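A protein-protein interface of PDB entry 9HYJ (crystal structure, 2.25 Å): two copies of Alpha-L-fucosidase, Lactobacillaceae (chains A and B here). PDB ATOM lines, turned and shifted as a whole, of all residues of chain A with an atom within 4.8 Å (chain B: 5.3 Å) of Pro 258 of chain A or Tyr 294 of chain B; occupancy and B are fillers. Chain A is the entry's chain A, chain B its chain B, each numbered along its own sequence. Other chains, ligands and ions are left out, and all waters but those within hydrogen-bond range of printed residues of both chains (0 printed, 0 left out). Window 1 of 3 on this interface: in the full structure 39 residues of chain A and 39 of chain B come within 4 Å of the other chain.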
ATOM      1  N   LYS A 256      28.404 -13.621 -15.179  1.00  0.00           N
ATOM      2  CA  LYS A 256      29.502 -14.535 -15.465  1.00  0.00           C
ATOM      3  C   LYS A 256      29.020 -15.613 -16.434  1.00  0.00           C
ATOM      4  O   LYS A 256      27.822 -15.854 -16.562  1.00  0.00           O
ATOM      5  CB  LYS A 256      29.898 -15.223 -14.157  1.00  0.00           C
ATOM      6  CG  LYS A 256      30.453 -14.244 -13.138  1.00  0.00           C
ATOM      7  CD  LYS A 256      30.677 -14.817 -11.739  1.00  0.00           C
ATOM      8  CE  LYS A 256      31.062 -13.701 -10.794  1.00  0.00           C
ATOM      9  NZ  LYS A 256      29.955 -12.727 -10.648  1.00  0.00           N
ATOM     10  N   SER A 257      29.959 -16.259 -17.137  1.00  0.00           N
ATOM     11  CA  SER A 257      29.555 -17.361 -17.995  1.00  0.00           C
ATOM     12  C   SER A 257      29.154 -18.560 -17.153  1.00  0.00           C
ATOM     13  O   SER A 257      29.717 -18.798 -16.083  1.00  0.00           O
ATOM     14  CB  SER A 257      30.612 -17.737 -19.000  1.00  0.00           C
ATOM     15  OG  SER A 257      31.734 -18.249 -18.317  1.00  0.00           O
ATOM     16  N   PRO A 258      28.167 -19.359 -17.598  1.00  0.00           N
ATOM     17  CA  PRO A 258      27.941 -20.675 -17.006  1.00  0.00           C
ATOM     18  C   PRO A 258      29.225 -21.502 -16.906  1.00  0.00           C
ATOM     19  O   PRO A 258      29.386 -22.261 -15.952  1.00  0.00           O
ATOM     20  CB  PRO A 258      26.914 -21.328 -17.930  1.00  0.00           C
ATOM     21  CG  PRO A 258      26.121 -20.072 -18.387  1.00  0.00           C
ATOM     22  CD  PRO A 258      27.181 -19.015 -18.630  1.00  0.00           C
ATOM     23  N   ALA A 259      30.142 -21.341 -17.876  1.00  0.00           N
ATOM     24  CA  ALA A 259      31.372 -22.115 -17.866  1.00  0.00           C
ATOM     25  C   ALA A 259      32.189 -21.725 -16.631  1.00  0.00           C
ATOM     26  O   ALA A 259      32.778 -22.582 -15.978  1.00  0.00           O
ATOM     27  CB  ALA A 259      32.195 -21.894 -19.166  1.00  0.00           C
ATOM     28  N   GLU A 260      32.261 -20.421 -16.343  1.00  0.00           N
ATOM     29  CA  GLU A 260      33.035 -19.972 -15.191  1.00  0.00           C
ATOM     30  C   GLU A 260      32.389 -20.475 -13.893  1.00  0.00           C
ATOM     31  O   GLU A 260      33.084 -20.826 -12.934  1.00  0.00           O
ATOM     32  CB  GLU A 260      33.159 -18.450 -15.181  1.00  0.00           C
ATOM     33  CG  GLU A 260      33.931 -17.969 -13.952  1.00  0.00           C
ATOM     34  CD  GLU A 260      34.105 -16.463 -13.739  1.00  0.00           C
ATOM     35  OE1 GLU A 260      33.748 -15.657 -14.633  1.00  0.00           O
ATOM     36  OE2 GLU A 260      34.493 -16.088 -12.621  1.00  0.00           O
ATOM     37  N   MET A 261      31.052 -20.527 -13.870  1.00  0.00           N
ATOM     38  CA  MET A 261      30.344 -21.074 -12.721  1.00  0.00           C
ATOM     39  C   MET A 261      30.787 -22.529 -12.484  1.00  0.00           C
ATOM     40  O   MET A 261      31.154 -22.910 -11.367  1.00  0.00           O
ATOM     41  CB  MET A 261      28.831 -20.969 -12.925  1.00  0.00           C
ATOM     42  CG  MET A 261      28.032 -21.676 -11.825  1.00  0.00           C
ATOM     43  SD  MET A 261      26.276 -21.706 -12.262  1.00  0.00           S
ATOM     44  CE  MET A 261      26.247 -22.531 -13.878  1.00  0.00           C
ATOM     45  N   ILE A 262      30.787 -23.341 -13.555  1.00  0.00           N
ATOM     46  CA  ILE A 262      31.175 -24.737 -13.438  1.00  0.00           C
ATOM     47  C   ILE A 262      32.632 -24.848 -12.971  1.00  0.00           C
ATOM     48  O   ILE A 262      32.930 -25.657 -12.091  1.00  0.00           O
ATOM     49  CB  ILE A 262      30.892 -25.498 -14.730  1.00  0.00           C
ATOM     50  CG1 ILE A 262      29.380 -25.710 -14.875  1.00  0.00           C
ATOM     51  CG2 ILE A 262      31.644 -26.844 -14.766  1.00  0.00           C
ATOM     52  CD1 ILE A 262      28.946 -26.117 -16.265  1.00  0.00           C
ATOM     53  N   TYR A 294      20.904 -20.697 -15.226  1.00  0.00           N
ATOM     54  CA  TYR A 294      22.178 -21.094 -14.636  1.00  0.00           C
ATOM     55  C   TYR A 294      22.006 -22.376 -13.837  1.00  0.00           C
ATOM     56  O   TYR A 294      22.875 -23.246 -13.891  1.00  0.00           O
ATOM     57  CB  TYR A 294      22.793 -19.986 -13.769  1.00  0.00           C
ATOM     58  CG  TYR A 294      23.492 -18.951 -14.635  1.00  0.00           C
ATOM     59  CD1 TYR A 294      22.759 -18.040 -15.382  1.00  0.00           C
ATOM     60  CD2 TYR A 294      24.881 -18.868 -14.689  1.00  0.00           C
ATOM     61  CE1 TYR A 294      23.387 -17.076 -16.158  1.00  0.00           C
ATOM     62  CE2 TYR A 294      25.529 -17.904 -15.462  1.00  0.00           C
ATOM     63  CZ  TYR A 294      24.773 -17.001 -16.189  1.00  0.00           C
ATOM     64  OH  TYR A 294      25.354 -16.072 -17.016  1.00  0.00           O
ATOM     65  N   LEU A 297      21.856 -25.396 -16.184  1.00  0.00           N
ATOM     66  CA  LEU A 297      23.133 -25.788 -16.748  1.00  0.00           C
ATOM     67  C   LEU A 297      23.997 -26.415 -15.663  1.00  0.00           C
ATOM     68  O   LEU A 297      24.598 -27.451 -15.905  1.00  0.00           O
ATOM     69  CB  LEU A 297      23.835 -24.594 -17.388  1.00  0.00           C
ATOM     70  CG  LEU A 297      23.098 -24.026 -18.607  1.00  0.00           C
ATOM     71  CD1 LEU A 297      23.668 -22.672 -18.984  1.00  0.00           C
ATOM     72  CD2 LEU A 297      23.044 -24.980 -19.809  1.00  0.00           C
ATOM     73  N   VAL B  69      14.615  -7.776 -28.405  1.00  0.00           N
ATOM     74  CA  VAL B  69      16.054  -7.797 -28.193  1.00  0.00           C
ATOM     75  C   VAL B  69      16.710  -6.622 -28.924  1.00  0.00           C
ATOM     76  O   VAL B  69      17.896  -6.355 -28.727  1.00  0.00           O
ATOM     77  CB  VAL B  69      16.694  -9.153 -28.548  1.00  0.00           C
ATOM     78  CG1 VAL B  69      16.893  -9.333 -30.044  1.00  0.00           C
ATOM     79  CG2 VAL B  69      18.061  -9.341 -27.906  1.00  0.00           C
ATOM     80  N   LEU B 242      25.645 -18.947 -28.606  1.00  0.00           N
ATOM     81  CA  LEU B 242      25.706 -18.780 -27.154  1.00  0.00           C
ATOM     82  C   LEU B 242      26.616 -19.807 -26.486  1.00  0.00           C
ATOM     83  O   LEU B 242      27.262 -19.482 -25.493  1.00  0.00           O
ATOM     84  CB  LEU B 242      24.298 -18.814 -26.545  1.00  0.00           C
ATOM     85  CG  LEU B 242      23.401 -17.655 -27.029  1.00  0.00           C
ATOM     86  CD1 LEU B 242      22.014 -17.810 -26.430  1.00  0.00           C
ATOM     87  CD2 LEU B 242      24.015 -16.204 -26.844  1.00  0.00           C
ATOM     88  N   LEU B 253      27.485 -27.240 -22.216  1.00  0.00           N
ATOM     89  CA  LEU B 253      27.330 -26.375 -21.053  1.00  0.00           C
ATOM     90  C   LEU B 253      28.253 -25.173 -21.175  1.00  0.00           C
ATOM     91  O   LEU B 253      28.293 -24.306 -20.290  1.00  0.00           O
ATOM     92  CB  LEU B 253      27.626 -27.145 -19.769  1.00  0.00           C
ATOM     93  CG  LEU B 253      26.877 -28.485 -19.626  1.00  0.00           C
ATOM     94  CD1 LEU B 253      27.141 -29.122 -18.282  1.00  0.00           C
ATOM     95  CD2 LEU B 253      25.378 -28.342 -19.835  1.00  0.00           C
ATOM     96  N   TYR B 255      28.569 -22.214 -22.276  1.00  0.00           N
ATOM     97  CA  TYR B 255      27.980 -20.940 -22.669  1.00  0.00           C
ATOM     98  C   TYR B 255      28.914 -19.770 -22.367  1.00  0.00           C
ATOM     99  O   TYR B 255      29.634 -19.772 -21.368  1.00  0.00           O
ATOM    100  CB  TYR B 255      26.705 -20.764 -21.849  1.00  0.00           C
ATOM    101  CG  TYR B 255      25.507 -21.469 -22.476  1.00  0.00           C
ATOM    102  CD1 TYR B 255      25.344 -22.854 -22.361  1.00  0.00           C
ATOM    103  CD2 TYR B 255      24.552 -20.745 -23.192  1.00  0.00           C
ATOM    104  CE1 TYR B 255      24.250 -23.503 -22.919  1.00  0.00           C
ATOM    105  CE2 TYR B 255      23.436 -21.370 -23.736  1.00  0.00           C
ATOM    106  CZ  TYR B 255      23.307 -22.750 -23.608  1.00  0.00           C
ATOM    107  OH  TYR B 255      22.235 -23.384 -24.124  1.00  0.00           O
ATOM    108  N   LYS B 256      28.905 -18.774 -23.260  1.00  0.00           N
ATOM    109  CA  LYS B 256      29.623 -17.515 -23.091  1.00  0.00           C
ATOM    110  C   LYS B 256      28.892 -16.663 -22.052  1.00  0.00           C
ATOM    111  O   LYS B 256      27.711 -16.880 -21.795  1.00  0.00           O
ATOM    112  CB  LYS B 256      29.599 -16.767 -24.425  1.00  0.00           C
ATOM    113  CG  LYS B 256      30.347 -17.502 -25.505  1.00  0.00           C
ATOM    114  CD  LYS B 256      30.327 -16.906 -26.905  1.00  0.00           C
ATOM    115  CE  LYS B 256      30.947 -17.840 -27.899  1.00  0.00           C
ATOM    116  NZ  LYS B 256      30.251 -19.141 -27.939  1.00  0.00           N
ATOM    117  N   SER B 257      29.597 -15.717 -21.433  1.00  0.00           N
ATOM    118  CA  SER B 257      28.913 -14.827 -20.506  1.00  0.00           C
ATOM    119  C   SER B 257      28.027 -13.856 -21.275  1.00  0.00           C
ATOM    120  O   SER B 257      28.349 -13.456 -22.397  1.00  0.00           O
ATOM    121  CB  SER B 257      29.863 -14.065 -19.610  1.00  0.00           C
ATOM    122  OG  SER B 257      30.652 -13.197 -20.378  1.00  0.00           O
ATOM    123  N   PRO B 258      26.871 -13.468 -20.713  1.00  0.00           N
ATOM    124  CA  PRO B 258      26.115 -12.351 -21.273  1.00  0.00           C
ATOM    125  C   PRO B 258      26.981 -11.103 -21.481  1.00  0.00           C
ATOM    126  O   PRO B 258      26.761 -10.345 -22.423  1.00  0.00           O
ATOM    127  CB  PRO B 258      24.992 -12.130 -20.246  1.00  0.00           C
ATOM    128  CG  PRO B 258      24.805 -13.554 -19.669  1.00  0.00           C
ATOM    129  CD  PRO B 258      26.199 -14.139 -19.587  1.00  0.00           C
ATOM    130  N   MET B 261      28.729 -11.389 -24.683  1.00  0.00           N
ATOM    131  CA  MET B 261      27.767 -11.149 -25.744  1.00  0.00           C
ATOM    132  C   MET B 261      27.621  -9.636 -25.996  1.00  0.00           C
ATOM    133  O   MET B 261      27.734  -9.183 -27.136  1.00  0.00           O
ATOM    134  CB  MET B 261      26.423 -11.802 -25.398  1.00  0.00           C
ATOM    135  CG  MET B 261      25.311 -11.425 -26.365  1.00  0.00           C
ATOM    136  SD  MET B 261      23.755 -12.101 -25.776  1.00  0.00           S
ATOM    137  CE  MET B 261      23.572 -11.292 -24.174  1.00  0.00           C
ATOM    138  N   ALA B 290      17.197 -21.004 -22.078  1.00  0.00           N
ATOM    139  CA  ALA B 290      18.526 -20.417 -21.959  1.00  0.00           C
ATOM    140  C   ALA B 290      18.678 -19.243 -22.924  1.00  0.00           C
ATOM    141  O   ALA B 290      19.229 -18.209 -22.568  1.00  0.00           O
ATOM    142  CB  ALA B 290      19.618 -21.462 -22.171  1.00  0.00           C
ATOM    143  N   ALA B 291      18.161 -19.400 -24.146  1.00  0.00           N
ATOM    144  CA  ALA B 291      18.279 -18.367 -25.154  1.00  0.00           C
ATOM    145  C   ALA B 291      17.456 -17.142 -24.739  1.00  0.00           C
ATOM    146  O   ALA B 291      17.883 -15.995 -24.941  1.00  0.00           O
ATOM    147  CB  ALA B 291      17.875 -18.922 -26.517  1.00  0.00           C
ATOM    148  N   GLN B 292      16.279 -17.388 -24.148  1.00  0.00           N
ATOM    149  CA  GLN B 292      15.437 -16.316 -23.630  1.00  0.00           C
ATOM    150  C   GLN B 292      16.212 -15.464 -22.610  1.00  0.00           C
ATOM    151  O   GLN B 292      16.152 -14.233 -22.671  1.00  0.00           O
ATOM    152  CB  GLN B 292      14.141 -16.792 -22.977  1.00  0.00           C
ATOM    153  CG  GLN B 292      13.052 -17.264 -23.931  1.00  0.00           C
ATOM    154  CD  GLN B 292      12.358 -16.179 -24.758  1.00  0.00           C
ATOM    155  OE1 GLN B 292      12.764 -15.009 -24.834  1.00  0.00           O
ATOM    156  NE2 GLN B 292      11.271 -16.558 -25.418  1.00  0.00           N
ATOM    157  N   THR B 293      16.962 -16.103 -21.692  1.00  0.00           N
ATOM    158  CA  THR B 293      17.733 -15.365 -20.697  1.00  0.00           C
ATOM    159  C   THR B 293      18.700 -14.398 -21.378  1.00  0.00           C
ATOM    160  O   THR B 293      18.754 -13.211 -21.039  1.00  0.00           O
ATOM    161  CB  THR B 293      18.436 -16.344 -19.751  1.00  0.00           C
ATOM    162  OG1 THR B 293      17.404 -16.919 -18.935  1.00  0.00           O
ATOM    163  CG2 THR B 293      19.474 -15.685 -18.865  1.00  0.00           C
ATOM    164  N   TYR B 294      19.442 -14.888 -22.375  1.00  0.00           N
ATOM    165  CA  TYR B 294      20.423 -14.061 -23.072  1.00  0.00           C
ATOM    166  C   TYR B 294      19.730 -12.931 -23.823  1.00  0.00           C
ATOM    167  O   TYR B 294      20.217 -11.799 -23.827  1.00  0.00           O
ATOM    168  CB  TYR B 294      21.319 -14.878 -23.993  1.00  0.00           C
ATOM    169  CG  TYR B 294      22.408 -15.592 -23.207  1.00  0.00           C
ATOM    170  CD1 TYR B 294      22.117 -16.711 -22.431  1.00  0.00           C
ATOM    171  CD2 TYR B 294      23.729 -15.165 -23.253  1.00  0.00           C
ATOM    172  CE1 TYR B 294      23.121 -17.388 -21.747  1.00  0.00           C
ATOM    173  CE2 TYR B 294      24.744 -15.834 -22.581  1.00  0.00           C
ATOM    174  CZ  TYR B 294      24.432 -16.942 -21.809  1.00  0.00           C
ATOM    175  OH  TYR B 294      25.399 -17.582 -21.069  1.00  0.00           O
ATOM    176  N   MET B 295      18.587 -13.239 -24.442  1.00  0.00           N
ATOM    177  CA  MET B 295      17.852 -12.215 -25.163  1.00  0.00           C
ATOM    178  C   MET B 295      17.341 -11.117 -24.235  1.00  0.00           C
ATOM    179  O   MET B 295      17.419  -9.936 -24.608  1.00  0.00           O
ATOM    180  CB  MET B 295      16.737 -12.816 -26.017  1.00  0.00           C
ATOM    181  CG  MET B 295      17.322 -13.528 -27.263  1.00  0.00           C
ATOM    182  SD  MET B 295      16.063 -14.586 -28.022  1.00  0.00           S
ATOM    183  CE  MET B 295      15.413 -13.203 -28.951  1.00  0.00           C
ATOM    184  N   HIS B 296      16.833 -11.503 -23.046  1.00  0.00           N
ATOM    185  CA  HIS B 296      16.374 -10.506 -22.080  1.00  0.00           C
ATOM    186  C   HIS B 296      17.519  -9.574 -21.665  1.00  0.00           C
ATOM    187  O   HIS B 296      17.341  -8.355 -21.605  1.00  0.00           O
ATOM    188  CB  HIS B 296      15.589 -11.132 -20.917  1.00  0.00           C
ATOM    189  CG  HIS B 296      14.270 -11.696 -21.375  1.00  0.00           C
ATOM    190  ND1 HIS B 296      13.669 -12.819 -20.838  1.00  0.00           N
ATOM    191  CD2 HIS B 296      13.445 -11.282 -22.352  1.00  0.00           C
ATOM    192  CE1 HIS B 296      12.537 -13.081 -21.484  1.00  0.00           C
ATOM    193  NE2 HIS B 296      12.390 -12.160 -22.407  1.00  0.00           N
ATOM    194  N   LEU B 297      18.701 -10.143 -21.398  1.00  0.00           N
ATOM    195  CA  LEU B 297      19.816  -9.306 -20.961  1.00  0.00           C
ATOM    196  C   LEU B 297      20.281  -8.409 -22.107  1.00  0.00           C
ATOM    197  O   LEU B 297      20.479  -7.221 -21.907  1.00  0.00           O
ATOM    198  CB  LEU B 297      20.966 -10.151 -20.411  1.00  0.00           C
ATOM    199  CG  LEU B 297      20.599 -10.950 -19.156  1.00  0.00           C
ATOM    200  CD1 LEU B 297      21.598 -12.058 -18.835  1.00  0.00           C
ATOM    201  CD2 LEU B 297      20.406 -10.027 -17.952  1.00  0.00           C
ATOM    202  N   LEU B 298      20.435  -8.987 -23.310  1.00  0.00           N
ATOM    203  CA  LEU B 298      20.887  -8.196 -24.436  1.00  0.00           C
ATOM    204  C   LEU B 298      19.870  -7.089 -24.736  1.00  0.00           C
ATOM    205  O   LEU B 298      20.251  -5.956 -25.017  1.00  0.00           O
ATOM    206  CB  LEU B 298      21.093  -9.082 -25.663  1.00  0.00           C
ATOM    207  CG  LEU B 298      21.575  -8.335 -26.912  1.00  0.00           C
ATOM    208  CD1 LEU B 298      22.882  -7.563 -26.602  1.00  0.00           C
ATOM    209  CD2 LEU B 298      21.774  -9.368 -28.002  1.00  0.00           C
ATOM    210  N   GLY B 299      18.573  -7.413 -24.605  1.00  0.00           N
ATOM    211  CA  GLY B 299      17.527  -6.437 -24.883  1.00  0.00           C
ATOM    212  C   GLY B 299      17.585  -5.220 -23.968  1.00  0.00           C
ATOM    213  O   GLY B 299      17.275  -4.111 -24.372  1.00  0.00           O
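The backbone carbonyl oxygen (O) of Lys 256 of chain A lies within hydrogen-bond range of the side-chain hydroxyl (OH) of Tyr 294 of chain A (2.5 Å). The backbone NH of Glu 260 of chain A sits at hydrogen-bond distance from the side-chain hydroxyl of Ser 257 of chain A (3.0 Å). N of Lys 256 of chain B sits at hydrogen-bond distance from O of Leu 242 of chain B, at 2.9 Å. OH of Tyr 294 of chain B lies within hydrogen-bond range of O of Lys 256 of chain B.
Lys 256 of chain A touches Ser 257 of chain B, and with the chains exchanged Ser 257 of chain A touches Lys 256 of chain B. Lys 256 of chain A touches Pro 258 of chain B, and with the chains exchanged Pro 258 of chain A touches Lys 256 of chain B. Ser 257 of chain B touches its own counterpart, Ser 257 of chain A. Pro 258 of chain A touches Tyr 294 of chain B, and with the chains exchanged Tyr 294 of chain A touches Pro 258 of chain B. 6 positions are printed for both chains. Of the 13 pairs that touch across the chains among the printed residues, 7 have their exchanged pair printed and touching as well.
Of the printed residues of chain B, Ala 259 of chain A touches Tyr 255. Of the printed residues of chain B, Ile 262 of chain A touches Leu 253. Of the printed residues of chain A, Lys 256 of chain B touches Ser 257 and Pro 258. Printed residues of chain A within 4 Å of Ser 257 of chain B: Lys 256 and Ser 257. Of chain A, only Pro 258 comes within 4 Å of Tyr 294 of chain B.
Among the printed residues, merely in contact across the chains: Lys 256 of chain A with Ser 257 of chain B, Lys 256 of chain A with Pro 258 of chain B, Ser 257 of chain A with Tyr 255 of chain B, Ser 257 of chain A with Lys 256 of chain B, Ser 257 of chain A with Ser 257 of chain B, Pro 258 of chain A with Tyr 255 of chain B, Pro 258 of chain A with Lys 256 of chain B, Pro 258 of chain A with Tyr 294 of chain B, Ala 259 of chain A with Tyr 255 of chain B, Ile 262 of chain A with Leu 253 of chain B, Tyr 294 of chain A with Pro 258 of chain B, Leu 297 of chain A with Leu 253 of chain B and Leu 297 of chain A with Tyr 255 of chain B.
Printed residues of chain B that touch a printed residue of chain A: Leu 253, Tyr 255, Lys 256, Ser 257, Pro 258 and Tyr 294. Hydrophobic or aromatic side chains of chain B within 4 Å of the printed part of chain A: Leu 253, Tyr 255, Pro 258 and Tyr 294. Of the 9 printed residues of chain A, 7 touch a printed residue of chain B. Hydrophobic or aromatic side chains of chain A that line the printed part of chain B: Pro 258, Ala 259, Ile 262, Tyr 294 and Leu 297. Along chain A the printed residues that touch a printed residue of chain B span positions 256 to 297. Among the printed residues, no Asp or Glu carboxylate lies within 4 Å of a Lys or Arg side-chain nitrogen of the other chain.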
